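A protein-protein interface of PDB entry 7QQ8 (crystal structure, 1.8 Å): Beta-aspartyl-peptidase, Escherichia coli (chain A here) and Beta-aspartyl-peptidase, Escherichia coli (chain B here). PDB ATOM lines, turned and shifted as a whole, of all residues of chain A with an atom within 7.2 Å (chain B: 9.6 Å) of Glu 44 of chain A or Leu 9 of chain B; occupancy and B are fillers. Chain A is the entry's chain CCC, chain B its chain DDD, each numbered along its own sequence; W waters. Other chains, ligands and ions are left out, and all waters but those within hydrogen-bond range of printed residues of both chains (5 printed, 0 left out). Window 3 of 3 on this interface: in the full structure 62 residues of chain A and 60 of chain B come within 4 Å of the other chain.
The backbone carbonyl oxygen of His 104 of chain B sits at hydrogen-bond distance from the side-chain amino group of Lys 3 of chain A, 2.9 Å away.
O of Ala 4 of chain A lies within hydrogen-bond range of N of Ala 124 of chain B (3.0 Å).
O of Val 5 of chain A is in hydrogen-bond range of N of Leu 7 of chain B, at 3.0 Å.
NE2 of Gln 40 of chain A sits at hydrogen-bond distance from O of Tyr 123 of chain B, 2.8 Å away.
NE2 of Gln 40 of chain A lies within hydrogen-bond range of O of Asp 126 of chain B.
The side-chain carboxylate of Asp 8 of chain B sits at hydrogen-bond distance from the backbone NH of Ala 49 of chain A.
O of Met 42 of chain A lies within hydrogen-bond range of N of Glu 47 of chain A (3.0 Å).
N of Asp 10 of chain B lies within hydrogen-bond range of OD1 of Asp 8 of chain B (2.9 Å).
N of Gly 11 of chain B is in hydrogen-bond range of OD1 of Asp 8 of chain B, 3.2 Å away.
N of Asn 12 of chain B is in hydrogen-bond range of OD1 of Asp 8 of chain B, 2.9 Å away.
Among the printed residues, pairs that only touch across the chains: Ala 4 of chain A with Leu 7 of chain B, Val 5 of chain A with Ala 6 of chain B, Ala 49 of chain A with Asn 12 of chain B, Ser 48 of chain A with Asp 8 of chain B, Ala 49 of chain A with Ala 6 of chain B, Gln 40 of chain A with Gly 122 of chain B, Val 5 of chain A with Gly 122 of chain B, Lys 3 of chain A with Leu 7 of chain B, Leu 43 of chain A with Leu 9 of chain B, Val 5 of chain A with Tyr 123 of chain B, Ala 4 of chain A with Tyr 123 of chain B, Glu 47 of chain A with Asp 8 of chain B, Ala 4 of chain A with Leu 9 of chain B, Leu 43 of chain A with Leu 7 of chain B, Leu 43 of chain A with Asp 8 of chain B, Glu 44 of chain A with Leu 9 of chain B and Val 52 of chain A with Ala 6 of chain B.
Glu 44 of chain A touches just one residue of chain B: Leu 9 (3.9 Å).
Printed residues of chain A within 4 Å of His 104 of chain B: Lys 3 (2.9 Å).
Of the printed residues of chain A, Asn 12 of chain B touches Ala 49 (3.3 Å).
Printed residues of chain A within 4 Å of Asp 126 of chain B: Gln 40 (2.9 Å).
Printed residues of chain A that touch a printed residue of chain B: Lys 3, Ala 4, Val 5, Gln 40, Leu 43, Glu 44, Glu 47, Ser 48, Ala 49 and Val 52.
Hydrophobic or aromatic side chains of chain A that line the printed part of chain B: Ala 4, Val 5, Leu 43, Ala 49 and Val 52.
Of the 15 printed residues of chain B, 10 touch a printed residue of chain A.
Among the printed residues, 23 pairs touch across the chains.
Among the printed residues, no Asp or Glu carboxylate lies within 4 Å of a Lys or Arg side-chain nitrogen of the other chain.
Water W1 lies within hydrogen-bond range of OE2 of Glu 44 of chain A (2.6 Å), N of Gly 125 of chain B (2.7 Å) and O of Gln 40 of chain A (3.2 Å).
Water W5 lies within hydrogen-bond range of O of Leu 43 of chain A, O of Glu 47 of chain A and N of Leu 9 of chain B.
Water W2 lies within hydrogen-bond range of O of His 104 of chain B (2.8 Å), NZ of Lys 3 of chain A (2.9 Å) and O of Gly 11 of chain B (3.4 Å).
Water W4 lies within hydrogen-bond range of O of Gly 46 of chain A (3.3 Å), OD2 of Asp 10 of chain B (3.4 Å) and N of Leu 9 of chain B (3.5 Å).
Water W3 bridges the backbone NH (N) of Ala 49 of chain A (3.3 Å) and the side-chain carboxylate (OD2) of Asp 8 of chain B (3.5 Å).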
ATOM      1  N   LYS A   3       8.861  21.281 -19.636  1.00  0.00           N
ATOM      2  CA  LYS A   3      10.292  21.239 -19.150  1.00  0.00           C
ATOM      3  C   LYS A   3      11.073  19.932 -19.451  1.00  0.00           C
ATOM      4  O   LYS A   3      12.131  19.780 -18.809  1.00  0.00           O
ATOM      5  CB  LYS A   3      10.294  21.404 -17.626  1.00  0.00           C
ATOM      6  CG  LYS A   3       9.650  20.252 -16.871  1.00  0.00           C
ATOM      7  CD  LYS A   3       9.571  20.445 -15.364  1.00  0.00           C
ATOM      8  CE  LYS A   3       8.978  19.218 -14.691  1.00  0.00           C
ATOM      9  NZ  LYS A   3       9.201  19.246 -13.225  1.00  0.00           N
ATOM     10  N   ALA A   4      10.679  19.051 -20.387  1.00  0.00           N
ATOM     11  CA  ALA A   4      11.482  17.845 -20.755  1.00  0.00           C
ATOM     12  C   ALA A   4      12.802  18.280 -21.389  1.00  0.00           C
ATOM     13  O   ALA A   4      12.772  19.269 -22.142  1.00  0.00           O
ATOM     14  CB  ALA A   4      10.743  16.901 -21.692  1.00  0.00           C
ATOM     15  N   VAL A   5      13.898  17.559 -21.137  1.00  0.00           N
ATOM     16  CA  VAL A   5      15.251  18.018 -21.530  1.00  0.00           C
ATOM     17  C   VAL A   5      16.220  16.835 -21.503  1.00  0.00           C
ATOM     18  O   VAL A   5      16.002  15.888 -20.691  1.00  0.00           O
ATOM     19  CB  VAL A   5      15.709  19.170 -20.611  1.00  0.00           C
ATOM     20  CG1 VAL A   5      15.694  18.816 -19.134  1.00  0.00           C
ATOM     21  CG2 VAL A   5      17.055  19.723 -21.027  1.00  0.00           C
ATOM     22  N   THR A  38      17.903  12.949 -31.511  1.00  0.00           N
ATOM     23  CA  THR A  38      17.097  11.722 -31.301  1.00  0.00           C
ATOM     24  C   THR A  38      16.452  11.731 -29.913  1.00  0.00           C
ATOM     25  O   THR A  38      15.262  11.420 -29.786  1.00  0.00           O
ATOM     26  CB  THR A  38      17.939  10.472 -31.508  1.00  0.00           C
ATOM     27  OG1 THR A  38      18.395  10.576 -32.855  1.00  0.00           O
ATOM     28  CG2 THR A  38      17.144   9.211 -31.242  1.00  0.00           C
ATOM     29  N   GLY A  39      17.212  12.076 -28.884  1.00  0.00           N
ATOM     30  CA  GLY A  39      16.694  12.157 -27.504  1.00  0.00           C
ATOM     31  C   GLY A  39      15.609  13.203 -27.352  1.00  0.00           C
ATOM     32  O   GLY A  39      14.570  12.888 -26.699  1.00  0.00           O
ATOM     33  N   GLN A  40      15.791  14.386 -27.947  1.00  0.00           N
ATOM     34  CA  GLN A  40      14.777  15.465 -27.846  1.00  0.00           C
ATOM     35  C   GLN A  40      13.476  14.971 -28.478  1.00  0.00           C
ATOM     36  O   GLN A  40      12.387  15.254 -27.928  1.00  0.00           O
ATOM     37  CB  GLN A  40      15.216  16.739 -28.561  1.00  0.00           C
ATOM     38  CG  GLN A  40      16.420  17.422 -27.940  1.00  0.00           C
ATOM     39  CD  GLN A  40      16.839  18.586 -28.814  1.00  0.00           C
ATOM     40  OE1 GLN A  40      17.574  18.417 -29.785  1.00  0.00           O
ATOM     41  NE2 GLN A  40      16.391  19.783 -28.455  1.00  0.00           N
ATOM     42  N   LYS A  41      13.586  14.283 -29.605  1.00  0.00           N
ATOM     43  CA  LYS A  41      12.402  13.850 -30.401  1.00  0.00           C
ATOM     44  C   LYS A  41      11.656  12.780 -29.610  1.00  0.00           C
ATOM     45  O   LYS A  41      10.380  12.897 -29.470  1.00  0.00           O
ATOM     46  CB  LYS A  41      12.850  13.323 -31.754  1.00  0.00           C
ATOM     47  CG  LYS A  41      13.288  14.404 -32.718  1.00  0.00           C
ATOM     48  CD  LYS A  41      14.003  13.888 -33.957  1.00  0.00           C
ATOM     49  CE  LYS A  41      14.363  14.985 -34.957  1.00  0.00           C
ATOM     50  NZ  LYS A  41      13.125  15.493 -35.608  1.00  0.00           N
ATOM     51  N   MET A  42      12.414  11.838 -29.035  1.00  0.00           N
ATOM     52  CA  MET A  42      11.843  10.798 -28.135  1.00  0.00           C
ATOM     53  C   MET A  42      11.129  11.473 -26.957  1.00  0.00           C
ATOM     54  O   MET A  42       9.938  11.181 -26.746  1.00  0.00           O
ATOM     55  CB  MET A  42      12.929   9.855 -27.619  1.00  0.00           C
ATOM     56  CG  MET A  42      13.459   8.951 -28.708  1.00  0.00           C
ATOM     57  SD  MET A  42      14.754   7.837 -28.188  1.00  0.00           S
ATOM     58  CE  MET A  42      13.811   6.744 -27.116  1.00  0.00           C
ATOM     59  N   LEU A  43      11.805  12.376 -26.239  1.00  0.00           N
ATOM     60  CA  LEU A  43      11.182  13.111 -25.090  1.00  0.00           C
ATOM     61  C   LEU A  43       9.892  13.808 -25.533  1.00  0.00           C
ATOM     62  O   LEU A  43       8.882  13.711 -24.831  1.00  0.00           O
ATOM     63  CB  LEU A  43      12.172  14.126 -24.495  1.00  0.00           C
ATOM     64  CG  LEU A  43      13.341  13.517 -23.708  1.00  0.00           C
ATOM     65  CD1 LEU A  43      14.327  14.595 -23.320  1.00  0.00           C
ATOM     66  CD2 LEU A  43      12.832  12.750 -22.475  1.00  0.00           C
ATOM     67  N   GLU A  44       9.939  14.498 -26.660  1.00  0.00           N
ATOM     68  CA  GLU A  44       8.812  15.319 -27.166  1.00  0.00           C
ATOM     69  C   GLU A  44       7.639  14.391 -27.486  1.00  0.00           C
ATOM     70  O   GLU A  44       6.491  14.791 -27.208  1.00  0.00           O
ATOM     71  CB  GLU A  44       9.285  16.129 -28.368  1.00  0.00           C
ATOM     72  CG  GLU A  44       8.392  17.294 -28.711  1.00  0.00           C
ATOM     73  CD  GLU A  44       8.438  17.597 -30.198  1.00  0.00           C
ATOM     74  OE1 GLU A  44       7.369  17.975 -30.783  1.00  0.00           O
ATOM     75  OE2 GLU A  44       9.554  17.410 -30.761  1.00  0.00           O
ATOM     76  N   ALA A  45       7.933  13.173 -27.940  1.00  0.00           N
ATOM     77  CA  ALA A  45       6.918  12.149 -28.294  1.00  0.00           C
ATOM     78  C   ALA A  45       6.456  11.435 -27.027  1.00  0.00           C
ATOM     79  O   ALA A  45       5.604  10.535 -27.168  1.00  0.00           O
ATOM     80  CB  ALA A  45       7.479  11.133 -29.266  1.00  0.00           C
ATOM     81  N   GLY A  46       7.019  11.757 -25.853  1.00  0.00           N
ATOM     82  CA  GLY A  46       6.546  11.203 -24.571  1.00  0.00           C
ATOM     83  C   GLY A  46       7.238   9.901 -24.174  1.00  0.00           C
ATOM     84  O   GLY A  46       6.737   9.241 -23.254  1.00  0.00           O
ATOM     85  N   GLU A  47       8.367   9.556 -24.791  1.00  0.00           N
ATOM     86  CA  GLU A  47       9.195   8.396 -24.349  1.00  0.00           C
ATOM     87  C   GLU A  47       9.782   8.689 -22.959  1.00  0.00           C
ATOM     88  O   GLU A  47       9.918   9.879 -22.613  1.00  0.00           O
ATOM     89  CB  GLU A  47      10.260   8.119 -25.405  1.00  0.00           C
ATOM     90  CG  GLU A  47       9.648   7.685 -26.714  1.00  0.00           C
ATOM     91  CD  GLU A  47       8.711   6.509 -26.594  1.00  0.00           C
ATOM     92  OE1 GLU A  47       7.576   6.581 -27.125  1.00  0.00           O
ATOM     93  OE2 GLU A  47       9.161   5.486 -26.095  1.00  0.00           O
ATOM     94  N   SER A  48      10.051   7.653 -22.169  1.00  0.00           N
ATOM     95  CA  SER A  48      10.560   7.757 -20.769  1.00  0.00           C
ATOM     96  C   SER A  48      12.008   8.259 -20.748  1.00  0.00           C
ATOM     97  O   SER A  48      12.797   7.924 -21.640  1.00  0.00           O
ATOM     98  CB  SER A  48      10.452   6.421 -20.064  1.00  0.00           C
ATOM     99  OG  SER A  48      11.355   5.478 -20.624  1.00  0.00           O
ATOM    100  N   ALA A  49      12.379   8.979 -19.705  1.00  0.00           N
ATOM    101  CA  ALA A  49      13.773   9.357 -19.421  1.00  0.00           C
ATOM    102  C   ALA A  49      14.669   8.108 -19.500  1.00  0.00           C
ATOM    103  O   ALA A  49      15.733   8.199 -20.054  1.00  0.00           O
ATOM    104  CB  ALA A  49      13.825  10.093 -18.095  1.00  0.00           C
ATOM    105  N   VAL A  52      15.086   7.007 -23.026  1.00  0.00           N
ATOM    106  CA  VAL A  52      15.855   8.107 -23.690  1.00  0.00           C
ATOM    107  C   VAL A  52      17.347   8.004 -23.343  1.00  0.00           C
ATOM    108  O   VAL A  52      18.198   8.042 -24.295  1.00  0.00           O
ATOM    109  CB  VAL A  52      15.307   9.505 -23.341  1.00  0.00           C
ATOM    110  CG1 VAL A  52      16.267  10.598 -23.730  1.00  0.00           C
ATOM    111  CG2 VAL A  52      13.982   9.769 -24.025  1.00  0.00           C
ATOM    112  N   ALA B   6      18.299  12.785 -18.524  1.00  0.00           N
ATOM    113  CA  ALA B   6      17.042  13.262 -19.107  1.00  0.00           C
ATOM    114  C   ALA B   6      16.000  13.442 -18.021  1.00  0.00           C
ATOM    115  O   ALA B   6      15.978  12.648 -17.059  1.00  0.00           O
ATOM    116  CB  ALA B   6      16.582  12.324 -20.180  1.00  0.00           C
ATOM    117  N   LEU B   7      15.138  14.434 -18.238  1.00  0.00           N
ATOM    118  CA  LEU B   7      13.861  14.621 -17.533  1.00  0.00           C
ATOM    119  C   LEU B   7      12.773  14.499 -18.596  1.00  0.00           C
ATOM    120  O   LEU B   7      12.865  15.225 -19.584  1.00  0.00           O
ATOM    121  CB  LEU B   7      13.892  16.013 -16.886  1.00  0.00           C
ATOM    122  CG  LEU B   7      12.597  16.492 -16.250  1.00  0.00           C
ATOM    123  CD1 LEU B   7      12.221  15.612 -15.074  1.00  0.00           C
ATOM    124  CD2 LEU B   7      12.693  17.979 -15.842  1.00  0.00           C
ATOM    125  N   ASP B   8      11.810  13.589 -18.402  1.00  0.00           N
ATOM    126  CA  ASP B   8      10.721  13.331 -19.359  1.00  0.00           C
ATOM    127  C   ASP B   8       9.477  14.151 -18.978  1.00  0.00           C
ATOM    128  O   ASP B   8       9.500  14.918 -17.982  1.00  0.00           O
ATOM    129  CB  ASP B   8      10.469  11.825 -19.485  1.00  0.00           C
ATOM    130  CG  ASP B   8       9.884  11.138 -18.270  1.00  0.00           C
ATOM    131  OD1 ASP B   8       9.244  11.830 -17.448  1.00  0.00           O
ATOM    132  OD2 ASP B   8      10.004   9.907 -18.196  1.00  0.00           O
ATOM    133  N   LEU B   9       8.422  13.998 -19.764  1.00  0.00           N
ATOM    134  CA  LEU B   9       7.183  14.818 -19.628  1.00  0.00           C
ATOM    135  C   LEU B   9       6.405  14.397 -18.384  1.00  0.00           C
ATOM    136  O   LEU B   9       5.525  15.185 -17.943  1.00  0.00           O
ATOM    137  CB  LEU B   9       6.342  14.644 -20.898  1.00  0.00           C
ATOM    138  CG  LEU B   9       6.879  15.335 -22.147  1.00  0.00           C
ATOM    139  CD1 LEU B   9       5.975  15.027 -23.320  1.00  0.00           C
ATOM    140  CD2 LEU B   9       7.019  16.837 -21.956  1.00  0.00           C
ATOM    141  N   ASP B  10       6.713  13.230 -17.826  1.00  0.00           N
ATOM    142  CA  ASP B  10       6.097  12.718 -16.579  1.00  0.00           C
ATOM    143  C   ASP B  10       6.879  13.195 -15.351  1.00  0.00           C
ATOM    144  O   ASP B  10       6.495  12.761 -14.253  1.00  0.00           O
ATOM    145  CB  ASP B  10       5.968  11.188 -16.622  1.00  0.00           C
ATOM    146  CG  ASP B  10       4.965  10.729 -17.661  1.00  0.00           C
ATOM    147  OD1 ASP B  10       4.075  11.533 -18.064  1.00  0.00           O
ATOM    148  OD2 ASP B  10       5.074   9.577 -18.048  1.00  0.00           O
ATOM    149  N   GLY B  11       7.936  14.010 -15.518  1.00  0.00           N
ATOM    150  CA  GLY B  11       8.779  14.448 -14.392  1.00  0.00           C
ATOM    151  C   GLY B  11       9.741  13.371 -13.914  1.00  0.00           C
ATOM    152  O   GLY B  11      10.264  13.520 -12.827  1.00  0.00           O
ATOM    153  N   ASN B  12       9.984  12.307 -14.677  1.00  0.00           N
ATOM    154  CA  ASN B  12      10.995  11.272 -14.317  1.00  0.00           C
ATOM    155  C   ASN B  12      12.395  11.695 -14.764  1.00  0.00           C
ATOM    156  O   ASN B  12      12.532  12.207 -15.900  1.00  0.00           O
ATOM    157  CB  ASN B  12      10.699   9.904 -14.936  1.00  0.00           C
ATOM    158  CG  ASN B  12       9.419   9.322 -14.410  1.00  0.00           C
ATOM    159  OD1 ASN B  12       9.206   9.313 -13.195  1.00  0.00           O
ATOM    160  ND2 ASN B  12       8.570   8.845 -15.315  1.00  0.00           N
ATOM    161  N   LEU B  13      13.384  11.443 -13.893  1.00  0.00           N
ATOM    162  CA  LEU B  13      14.828  11.651 -14.150  1.00  0.00           C
ATOM    163  C   LEU B  13      15.486  10.295 -14.370  1.00  0.00           C
ATOM    164  O   LEU B  13      15.110   9.361 -13.678  1.00  0.00           O
ATOM    165  CB  LEU B  13      15.455  12.374 -12.961  1.00  0.00           C
ATOM    166  CG  LEU B  13      15.143  13.873 -12.879  1.00  0.00           C
ATOM    167  CD1 LEU B  13      15.597  14.456 -11.522  1.00  0.00           C
ATOM    168  CD2 LEU B  13      15.776  14.621 -14.031  1.00  0.00           C
ATOM    169  N   HIS B 104      15.205  18.164 -10.953  1.00  0.00           N
ATOM    170  CA  HIS B 104      13.752  17.863 -10.998  1.00  0.00           C
ATOM    171  C   HIS B 104      12.988  19.080 -11.523  1.00  0.00           C
ATOM    172  O   HIS B 104      11.825  18.882 -11.931  1.00  0.00           O
ATOM    173  CB  HIS B 104      13.232  17.399  -9.628  1.00  0.00           C
ATOM    174  CG  HIS B 104      13.251  18.430  -8.541  1.00  0.00           C
ATOM    175  ND1 HIS B 104      12.141  19.201  -8.242  1.00  0.00           N
ATOM    176  CD2 HIS B 104      14.220  18.806  -7.665  1.00  0.00           C
ATOM    177  CE1 HIS B 104      12.449  20.032  -7.252  1.00  0.00           C
ATOM    178  NE2 HIS B 104      13.729  19.821  -6.891  1.00  0.00           N
ATOM    179  N   GLY B 122      19.518  19.800 -25.034  1.00  0.00           N
ATOM    180  CA  GLY B 122      18.382  20.485 -25.665  1.00  0.00           C
ATOM    181  C   GLY B 122      17.107  20.234 -24.902  1.00  0.00           C
ATOM    182  O   GLY B 122      16.867  19.088 -24.471  1.00  0.00           O
ATOM    183  N   TYR B 123      16.309  21.282 -24.773  1.00  0.00           N
ATOM    184  CA  TYR B 123      14.893  21.207 -24.360  1.00  0.00           C
ATOM    185  C   TYR B 123      14.134  20.475 -25.481  1.00  0.00           C
ATOM    186  O   TYR B 123      14.472  20.616 -26.658  1.00  0.00           O
ATOM    187  CB  TYR B 123      14.430  22.621 -23.978  1.00  0.00           C
ATOM    188  CG  TYR B 123      15.022  23.110 -22.678  1.00  0.00           C
ATOM    189  CD1 TYR B 123      14.686  22.474 -21.500  1.00  0.00           C
ATOM    190  CD2 TYR B 123      15.902  24.184 -22.595  1.00  0.00           C
ATOM    191  CE1 TYR B 123      15.222  22.850 -20.285  1.00  0.00           C
ATOM    192  CE2 TYR B 123      16.429  24.595 -21.375  1.00  0.00           C
ATOM    193  CZ  TYR B 123      16.108  23.899 -20.212  1.00  0.00           C
ATOM    194  OH  TYR B 123      16.573  24.202 -18.951  1.00  0.00           O
ATOM    195  N   ALA B 124      13.145  19.665 -25.112  1.00  0.00           N
ATOM    196  CA  ALA B 124      12.180  19.062 -26.063  1.00  0.00           C
ATOM    197  C   ALA B 124      11.466  20.220 -26.772  1.00  0.00           C
ATOM    198  O   ALA B 124      11.034  21.167 -26.085  1.00  0.00           O
ATOM    199  CB  ALA B 124      11.185  18.169 -25.341  1.00  0.00           C
ATOM    200  N   GLY B 125      11.373  20.170 -28.094  1.00  0.00           N
ATOM    201  CA  GLY B 125      10.711  21.230 -28.887  1.00  0.00           C
ATOM    202  C   GLY B 125      11.595  22.459 -29.047  1.00  0.00           C
ATOM    203  O   GLY B 125      11.102  23.462 -29.616  1.00  0.00           O
ATOM    204  N   ASP B 126      12.875  22.382 -28.661  1.00  0.00           N
ATOM    205  CA  ASP B 126      13.811  23.517 -28.837  1.00  0.00           C
ATOM    206  C   ASP B 126      14.983  23.020 -29.676  1.00  0.00           C
ATOM    207  O   ASP B 126      14.994  21.856 -30.002  1.00  0.00           O
ATOM    208  CB  ASP B 126      14.137  24.118 -27.478  1.00  0.00           C
ATOM    209  CG  ASP B 126      14.277  25.624 -27.514  1.00  0.00           C
ATOM    210  OD1 ASP B 126      14.701  26.123 -28.547  1.00  0.00           O
ATOM    211  OD2 ASP B 126      13.918  26.285 -26.520  1.00  0.00           O
ATOM    212  N   THR B 127      15.880  23.904 -30.098  1.00  0.00           N
ATOM    213  CA  THR B 127      17.079  23.529 -30.896  1.00  0.00           C
ATOM    214  C   THR B 127      18.181  23.113 -29.921  1.00  0.00           C
ATOM    215  O   THR B 127      18.316  23.683 -28.836  1.00  0.00           O
ATOM    216  CB  THR B 127      17.490  24.659 -31.851  1.00  0.00           C
ATOM    217  OG1 THR B 127      17.929  25.773 -31.080  1.00  0.00           O
ATOM    218  CG2 THR B 127      16.360  25.150 -32.723  1.00  0.00           C
HETATM  219  O   HOH W   1      11.767  17.958 -29.606  1.00  0.00           O
HETATM  220  O   HOH W   2       9.999  16.785 -11.899  1.00  0.00           O
HETATM  221  O   HOH W   3      11.787   7.152 -16.981  1.00  0.00           O
HETATM  222  O   HOH W   4       7.332  10.758 -20.369  1.00  0.00           O
HETATM  223  O   HOH W   5       8.872  12.579 -22.340  1.00  0.00           O
